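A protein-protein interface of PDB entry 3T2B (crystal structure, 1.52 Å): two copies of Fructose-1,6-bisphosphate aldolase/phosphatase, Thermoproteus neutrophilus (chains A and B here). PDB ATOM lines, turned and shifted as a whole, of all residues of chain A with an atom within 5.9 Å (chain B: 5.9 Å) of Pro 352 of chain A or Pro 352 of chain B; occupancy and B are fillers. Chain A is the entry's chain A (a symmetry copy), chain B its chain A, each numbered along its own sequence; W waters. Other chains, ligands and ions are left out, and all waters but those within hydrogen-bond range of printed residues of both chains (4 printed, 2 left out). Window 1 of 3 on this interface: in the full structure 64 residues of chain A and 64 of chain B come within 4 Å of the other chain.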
ATOM      1  N   HIS A 262     -31.572  14.419  -3.405  1.00  0.00           N
ATOM      2  CA  HIS A 262     -31.892  15.285  -4.561  1.00  0.00           C
ATOM      3  C   HIS A 262     -33.309  15.559  -4.741  1.00  0.00           C
ATOM      4  O   HIS A 262     -34.175  14.587  -4.616  1.00  0.00           O
ATOM      5  CB  HIS A 262     -31.406  14.578  -5.847  1.00  0.00           C
ATOM      6  CG  HIS A 262     -29.935  14.380  -6.012  1.00  0.00           C
ATOM      7  ND1 HIS A 262     -28.925  14.794  -5.165  1.00  0.00           N
ATOM      8  CD2 HIS A 262     -29.315  13.799  -7.069  1.00  0.00           C
ATOM      9  CE1 HIS A 262     -27.740  14.465  -5.680  1.00  0.00           C
ATOM     10  NE2 HIS A 262     -27.957  13.823  -6.809  1.00  0.00           N
ATOM     11  N   GLN A 347     -23.871  24.567  -7.337  1.00  0.00           N
ATOM     12  CA  GLN A 347     -23.524  23.177  -7.003  1.00  0.00           C
ATOM     13  C   GLN A 347     -22.618  23.189  -5.798  1.00  0.00           C
ATOM     14  O   GLN A 347     -21.785  24.067  -5.652  1.00  0.00           O
ATOM     15  CB  GLN A 347     -22.747  22.438  -8.096  1.00  0.00           C
ATOM     16  CG  GLN A 347     -23.650  22.005  -9.223  1.00  0.00           C
ATOM     17  CD  GLN A 347     -22.831  21.142 -10.171  1.00  0.00           C
ATOM     18  OE1 GLN A 347     -22.470  21.654 -11.209  1.00  0.00           O
ATOM     19  NE2 GLN A 347     -22.628  19.881  -9.895  1.00  0.00           N
ATOM     20  N   ARG A 350     -27.365  23.339  -5.698  1.00  0.00           N
ATOM     21  CA  ARG A 350     -28.064  23.128  -6.986  1.00  0.00           C
ATOM     22  C   ARG A 350     -27.472  21.846  -7.571  1.00  0.00           C
ATOM     23  O   ARG A 350     -26.275  21.542  -7.407  1.00  0.00           O
ATOM     24  CB  ARG A 350     -27.685  24.288  -7.881  1.00  0.00           C
ATOM     25  CG  ARG A 350     -28.702  24.438  -9.054  1.00  0.00           C
ATOM     26  CD  ARG A 350     -27.916  24.884 -10.339  1.00  0.00           C
ATOM     27  NE  ARG A 350     -27.138  23.799 -10.856  1.00  0.00           N
ATOM     28  CZ  ARG A 350     -26.164  23.951 -11.773  1.00  0.00           C
ATOM     29  NH1 ARG A 350     -25.557  22.856 -12.192  1.00  0.00           N
ATOM     30  NH2 ARG A 350     -25.884  25.198 -12.264  1.00  0.00           N
ATOM     31  N   LEU A 351     -28.361  21.047  -8.254  1.00  0.00           N
ATOM     32  CA  LEU A 351     -27.900  19.756  -8.762  1.00  0.00           C
ATOM     33  C   LEU A 351     -27.015  19.862 -10.004  1.00  0.00           C
ATOM     34  O   LEU A 351     -27.000  20.921 -10.621  1.00  0.00           O
ATOM     35  CB  LEU A 351     -29.096  18.894  -9.120  1.00  0.00           C
ATOM     36  CG  LEU A 351     -29.903  18.480  -7.822  1.00  0.00           C
ATOM     37  CD1 LEU A 351     -31.115  17.600  -8.247  1.00  0.00           C
ATOM     38  CD2 LEU A 351     -29.056  17.828  -6.739  1.00  0.00           C
ATOM     39  N   PRO A 352     -26.280  18.803 -10.313  1.00  0.00           N
ATOM     40  CA  PRO A 352     -25.489  18.749 -11.549  1.00  0.00           C
ATOM     41  C   PRO A 352     -26.453  18.981 -12.766  1.00  0.00           C
ATOM     42  O   PRO A 352     -27.623  18.703 -12.742  1.00  0.00           O
ATOM     43  CB  PRO A 352     -24.921  17.324 -11.528  1.00  0.00           C
ATOM     44  CG  PRO A 352     -25.046  16.846 -10.184  1.00  0.00           C
ATOM     45  CD  PRO A 352     -26.219  17.533  -9.568  1.00  0.00           C
ATOM     46  N   PRO A 353     -25.926  19.580 -13.830  1.00  0.00           N
ATOM     47  CA  PRO A 353     -26.818  20.141 -14.818  1.00  0.00           C
ATOM     48  C   PRO A 353     -27.741  19.098 -15.526  1.00  0.00           C
ATOM     49  O   PRO A 353     -28.900  19.407 -15.754  1.00  0.00           O
ATOM     50  CB  PRO A 353     -25.816  20.850 -15.796  1.00  0.00           C
ATOM     51  CG  PRO A 353     -24.429  20.253 -15.487  1.00  0.00           C
ATOM     52  CD  PRO A 353     -24.491  19.879 -13.996  1.00  0.00           C
ATOM     53  N   GLU A 354     -27.262  17.881 -15.648  1.00  0.00           N
ATOM     54  CA  GLU A 354     -28.050  16.839 -16.282  1.00  0.00           C
ATOM     55  C   GLU A 354     -28.997  16.180 -15.309  1.00  0.00           C
ATOM     56  O   GLU A 354     -29.851  15.416 -15.735  1.00  0.00           O
ATOM     57  CB  GLU A 354     -27.175  15.754 -16.923  1.00  0.00           C
ATOM     58  CG  GLU A 354     -25.662  15.937 -16.848  1.00  0.00           C
ATOM     59  CD  GLU A 354     -25.164  15.907 -15.381  1.00  0.00           C
ATOM     60  OE1 GLU A 354     -25.443  14.891 -14.690  1.00  0.00           O
ATOM     61  OE2 GLU A 354     -24.485  16.851 -14.959  1.00  0.00           O
ATOM     62  N   GLU A 355     -28.849  16.468 -14.005  1.00  0.00           N
ATOM     63  CA  GLU A 355     -29.789  15.972 -12.947  1.00  0.00           C
ATOM     64  C   GLU A 355     -30.885  16.916 -12.575  1.00  0.00           C
ATOM     65  O   GLU A 355     -31.826  16.494 -11.892  1.00  0.00           O
ATOM     66  CB  GLU A 355     -29.009  15.505 -11.689  1.00  0.00           C
ATOM     67  CG  GLU A 355     -27.913  14.489 -12.088  1.00  0.00           C
ATOM     68  CD  GLU A 355     -27.330  13.648 -10.907  1.00  0.00           C
ATOM     69  OE1 GLU A 355     -26.062  13.611 -10.743  1.00  0.00           O
ATOM     70  OE2 GLU A 355     -28.148  12.963 -10.227  1.00  0.00           O
ATOM     71  N   MET A 356     -30.855  18.172 -13.042  1.00  0.00           N
ATOM     72  CA  MET A 356     -31.892  19.133 -12.615  1.00  0.00           C
ATOM     73  C   MET A 356     -33.104  19.003 -13.474  1.00  0.00           C
ATOM     74  O   MET A 356     -32.997  18.827 -14.674  1.00  0.00           O
ATOM     75  CB  MET A 356     -31.431  20.613 -12.583  1.00  0.00           C
ATOM     76  CG  MET A 356     -30.495  21.099 -13.668  1.00  0.00           C
ATOM     77  SD  MET A 356     -29.352  22.369 -12.964  1.00  0.00           S
ATOM     78  CE  MET A 356     -30.540  23.646 -12.598  1.00  0.00           C
ATOM     79  N   HIS B 262     -16.380  21.082  -4.244  1.00  0.00           N
ATOM     80  CA  HIS B 262     -15.949  19.755  -4.737  1.00  0.00           C
ATOM     81  C   HIS B 262     -14.531  19.478  -4.571  1.00  0.00           C
ATOM     82  O   HIS B 262     -13.654  20.404  -4.859  1.00  0.00           O
ATOM     83  CB  HIS B 262     -16.246  19.679  -6.252  1.00  0.00           C
ATOM     84  CG  HIS B 262     -17.677  19.712  -6.677  1.00  0.00           C
ATOM     85  ND1 HIS B 262     -18.799  19.760  -5.871  1.00  0.00           N
ATOM     86  CD2 HIS B 262     -18.140  19.642  -7.950  1.00  0.00           C
ATOM     87  CE1 HIS B 262     -19.898  19.734  -6.625  1.00  0.00           C
ATOM     88  NE2 HIS B 262     -19.520  19.707  -7.886  1.00  0.00           N
ATOM     89  N   GLN B 347     -23.879  10.101  -3.291  1.00  0.00           N
ATOM     90  CA  GLN B 347     -24.217  11.450  -3.770  1.00  0.00           C
ATOM     91  C   GLN B 347     -25.266  12.031  -2.856  1.00  0.00           C
ATOM     92  O   GLN B 347     -26.141  11.327  -2.382  1.00  0.00           O
ATOM     93  CB  GLN B 347     -24.826  11.492  -5.174  1.00  0.00           C
ATOM     94  CG  GLN B 347     -23.775  11.311  -6.240  1.00  0.00           C
ATOM     95  CD  GLN B 347     -24.439  11.531  -7.590  1.00  0.00           C
ATOM     96  OE1 GLN B 347     -24.685  10.544  -8.251  1.00  0.00           O
ATOM     97  NE2 GLN B 347     -24.631  12.746  -8.034  1.00  0.00           N
ATOM     98  N   ARG B 350     -20.577  12.120  -2.103  1.00  0.00           N
ATOM     99  CA  ARG B 350     -19.716  11.659  -3.216  1.00  0.00           C
ATOM    100  C   ARG B 350     -20.185  12.433  -4.447  1.00  0.00           C
ATOM    101  O   ARG B 350     -21.382  12.736  -4.615  1.00  0.00           O
ATOM    102  CB  ARG B 350     -20.020  10.192  -3.422  1.00  0.00           C
ATOM    103  CG  ARG B 350     -18.871   9.493  -4.211  1.00  0.00           C
ATOM    104  CD  ARG B 350     -19.506   8.420  -5.167  1.00  0.00           C
ATOM    105  NE  ARG B 350     -20.175   9.054  -6.262  1.00  0.00           N
ATOM    106  CZ  ARG B 350     -21.033   8.416  -7.082  1.00  0.00           C
ATOM    107  NH1 ARG B 350     -21.544   9.115  -8.078  1.00  0.00           N
ATOM    108  NH2 ARG B 350     -21.292   7.086  -6.888  1.00  0.00           N
ATOM    109  N   LEU B 351     -19.191  12.795  -5.327  1.00  0.00           N
ATOM    110  CA  LEU B 351     -19.540  13.620  -6.483  1.00  0.00           C
ATOM    111  C   LEU B 351     -20.267  12.858  -7.590  1.00  0.00           C
ATOM    112  O   LEU B 351     -20.241  11.633  -7.567  1.00  0.00           O
ATOM    113  CB  LEU B 351     -18.279  14.215  -7.082  1.00  0.00           C
ATOM    114  CG  LEU B 351     -17.626  15.268  -6.096  1.00  0.00           C
ATOM    115  CD1 LEU B 351     -16.340  15.844  -6.760  1.00  0.00           C
ATOM    116  CD2 LEU B 351     -18.579  16.355  -5.621  1.00  0.00           C
ATOM    117  N   PRO B 352     -20.920  13.579  -8.490  1.00  0.00           N
ATOM    118  CA  PRO B 352     -21.548  12.958  -9.664  1.00  0.00           C
ATOM    119  C   PRO B 352     -20.449  12.165 -10.455  1.00  0.00           C
ATOM    120  O   PRO B 352     -19.282  12.456 -10.432  1.00  0.00           O
ATOM    121  CB  PRO B 352     -22.064  14.169 -10.452  1.00  0.00           C
ATOM    122  CG  PRO B 352     -22.092  15.276  -9.546  1.00  0.00           C
ATOM    123  CD  PRO B 352     -21.029  15.048  -8.523  1.00  0.00           C
ATOM    124  N   PRO B 353     -20.860  11.085 -11.112  1.00  0.00           N
ATOM    125  CA  PRO B 353     -19.872  10.125 -11.548  1.00  0.00           C
ATOM    126  C   PRO B 353     -18.832  10.684 -12.572  1.00  0.00           C
ATOM    127  O   PRO B 353     -17.665  10.342 -12.461  1.00  0.00           O
ATOM    128  CB  PRO B 353     -20.769   8.979 -12.135  1.00  0.00           C
ATOM    129  CG  PRO B 353     -22.161   9.600 -12.355  1.00  0.00           C
ATOM    130  CD  PRO B 353     -22.272  10.693 -11.277  1.00  0.00           C
ATOM    131  N   GLU B 354     -19.250  11.645 -13.363  1.00  0.00           N
ATOM    132  CA  GLU B 354     -18.353  12.236 -14.341  1.00  0.00           C
ATOM    133  C   GLU B 354     -17.512  13.336 -13.740  1.00  0.00           C
ATOM    134  O   GLU B 354     -16.586  13.799 -14.388  1.00  0.00           O
ATOM    135  CB  GLU B 354     -19.103  12.803 -15.553  1.00  0.00           C
ATOM    136  CG  GLU B 354     -20.620  12.633 -15.584  1.00  0.00           C
ATOM    137  CD  GLU B 354     -21.295  13.399 -14.418  1.00  0.00           C
ATOM    138  OE1 GLU B 354     -21.069  14.635 -14.323  1.00  0.00           O
ATOM    139  OE2 GLU B 354     -22.053  12.786 -13.658  1.00  0.00           O
ATOM    140  N   GLU B 355     -17.832  13.758 -12.505  1.00  0.00           N
ATOM    141  CA  GLU B 355     -17.014  14.762 -11.747  1.00  0.00           C
ATOM    142  C   GLU B 355     -16.006  14.185 -10.808  1.00  0.00           C
ATOM    143  O   GLU B 355     -15.143  14.931 -10.330  1.00  0.00           O
ATOM    144  CB  GLU B 355     -17.927  15.785 -11.020  1.00  0.00           C
ATOM    145  CG  GLU B 355     -18.929  16.409 -12.020  1.00  0.00           C
ATOM    146  CD  GLU B 355     -19.625  17.718 -11.526  1.00  0.00           C
ATOM    147  OE1 GLU B 355     -20.901  17.790 -11.564  1.00  0.00           O
ATOM    148  OE2 GLU B 355     -18.875  18.684 -11.202  1.00  0.00           O
ATOM    149  N   MET B 356     -16.021  12.868 -10.558  1.00  0.00           N
ATOM    150  CA  MET B 356     -15.080  12.303  -9.571  1.00  0.00           C
ATOM    151  C   MET B 356     -13.767  12.012 -10.215  1.00  0.00           C
ATOM    152  O   MET B 356     -13.717  11.539 -11.336  1.00  0.00           O
ATOM    153  CB  MET B 356     -15.592  11.037  -8.837  1.00  0.00           C
ATOM    154  CG  MET B 356     -16.403  10.027  -9.621  1.00  0.00           C
ATOM    155  SD  MET B 356     -17.668   9.265  -8.511  1.00  0.00           S
ATOM    156  CE  MET B 356     -16.580   8.403  -7.393  1.00  0.00           C
HETATM  157  O   HOH W   1     -19.989  20.925 -12.181  1.00  0.00           O
HETATM  158  O   HOH W   2     -27.000  10.579  -9.759  1.00  0.00           O
HETATM  159  O   HOH W   3     -22.379  18.427  -7.201  1.00  0.00           O
HETATM  160  O   HOH W   4     -25.162  15.372  -6.534  1.00  0.00           O
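Among the printed residues, merely in contact across the chains: His 262 of chain A with Gln 347 of chain B (3.7 Å), Gln 347 of chain A with His 262 of chain B (3.7 Å) and Pro 352 of chain A with Pro 352 of chain B (3.4 Å).
The side-chain amide nitrogen of Gln 347 of chain B sits at hydrogen-bond distance from the side-chain carboxylate of Glu 355 of chain A (3.2 Å).
The side-chain amide nitrogen (NE2) of Gln 347 of chain A lies within hydrogen-bond range of the side-chain carboxylate (OE1) of Glu 355 of chain B (3.2 Å).
His 262 of chain A touches Gln 347 of chain B, and with the chains exchanged Gln 347 of chain A touches His 262 of chain B.
Gln 347 of chain A touches Glu 355 of chain B, and with the chains exchanged Glu 355 of chain A touches Gln 347 of chain B.
Pro 352 of chain B touches its own counterpart, Pro 352 of chain A.
9 positions are printed for both chains.
Of the 5 pairs that touch across the chains among the printed residues, 5 have their exchanged pair printed and touching as well.
The side-chain amide oxygen (OE1) of Gln 347 of chain B lies within hydrogen-bond range of the guanidinium group (NH1) of Arg 350 of chain B (3.5 Å).
OE1 of Gln 347 of chain A is in hydrogen-bond range of NH1 of Arg 350 of chain A, 3.5 Å away.
Water W2 lies within hydrogen-bond range of OE2 of Glu 355 of chain A (2.7 Å) and OE1 of Gln 347 of chain B (2.8 Å).
Water W1 bridges OE2 of Glu 355 of chain B (2.7 Å) and OE1 of Gln 347 of chain A (2.8 Å).
Water W4 lies within hydrogen-bond range of NE2 of Gln 347 of chain B (3.1 Å) and NE2 of His 262 of chain A (3.2 Å).
Water W3 bridges the side-chain amide nitrogen (NE2) of Gln 347 of chain A (3.1 Å) and a ring nitrogen (NE2) of His 262 of chain B (3.2 Å).
Hydrophobic or aromatic side chains of chain B within 4 Å of the printed part of chain A: His 262 and Pro 352.
Along chain B the printed residues that touch a printed residue of chain A span positions 262 to 355.
Printed residues of chain A that touch a printed residue of chain B: His 262, Gln 347, Pro 352 and Glu 355.
Hydrophobic or aromatic side chains of chain A that line the printed part of chain B: His 262 and Pro 352.
Among the printed residues, 5 pairs touch across the chains.
Among the printed residues, no Asp or Glu carboxylate lies within 4 Å of a Lys or Arg side-chain nitrogen of the other chain.
Pro 352 of chain A touches just one residue of chain B: Pro 352 (3.4 Å).
Of chain A, only Pro 352 (3.4 Å) comes within 4 Å of Pro 352 of chain B.
Of the printed residues of chain A, His 262 of chain B touches Gln 347.
Printed residues of chain B within 4 Å of Glu 355 of chain A: Gln 347.
Of the printed residues of chain B, His 262 of chain A touches Gln 347 (3.7 Å).
Printed residues of chain A within 4 Å of Glu 355 of chain B: Gln 347 (3.2 Å).
Of the printed residues of chain B, Gln 347 of chain A touches His 262 (3.7 Å) and Glu 355 (3.2 Å).
Arg 350 of chain B touches none of the printed residues of chain A.
Glu 354 of chain B touches none of the printed residues of chain A.
The nearest residue of chain B that does not touch Pro 352 of chain A is Glu 355 of chain B (4.05 Å).
The nearest residue of chain A that does not touch Pro 352 of chain B is Glu 355 of chain A (4.05 Å).
The nearest printed residue of chain B that does not touch His 262 of chain A is Pro 352 of chain B (6.6 Å).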
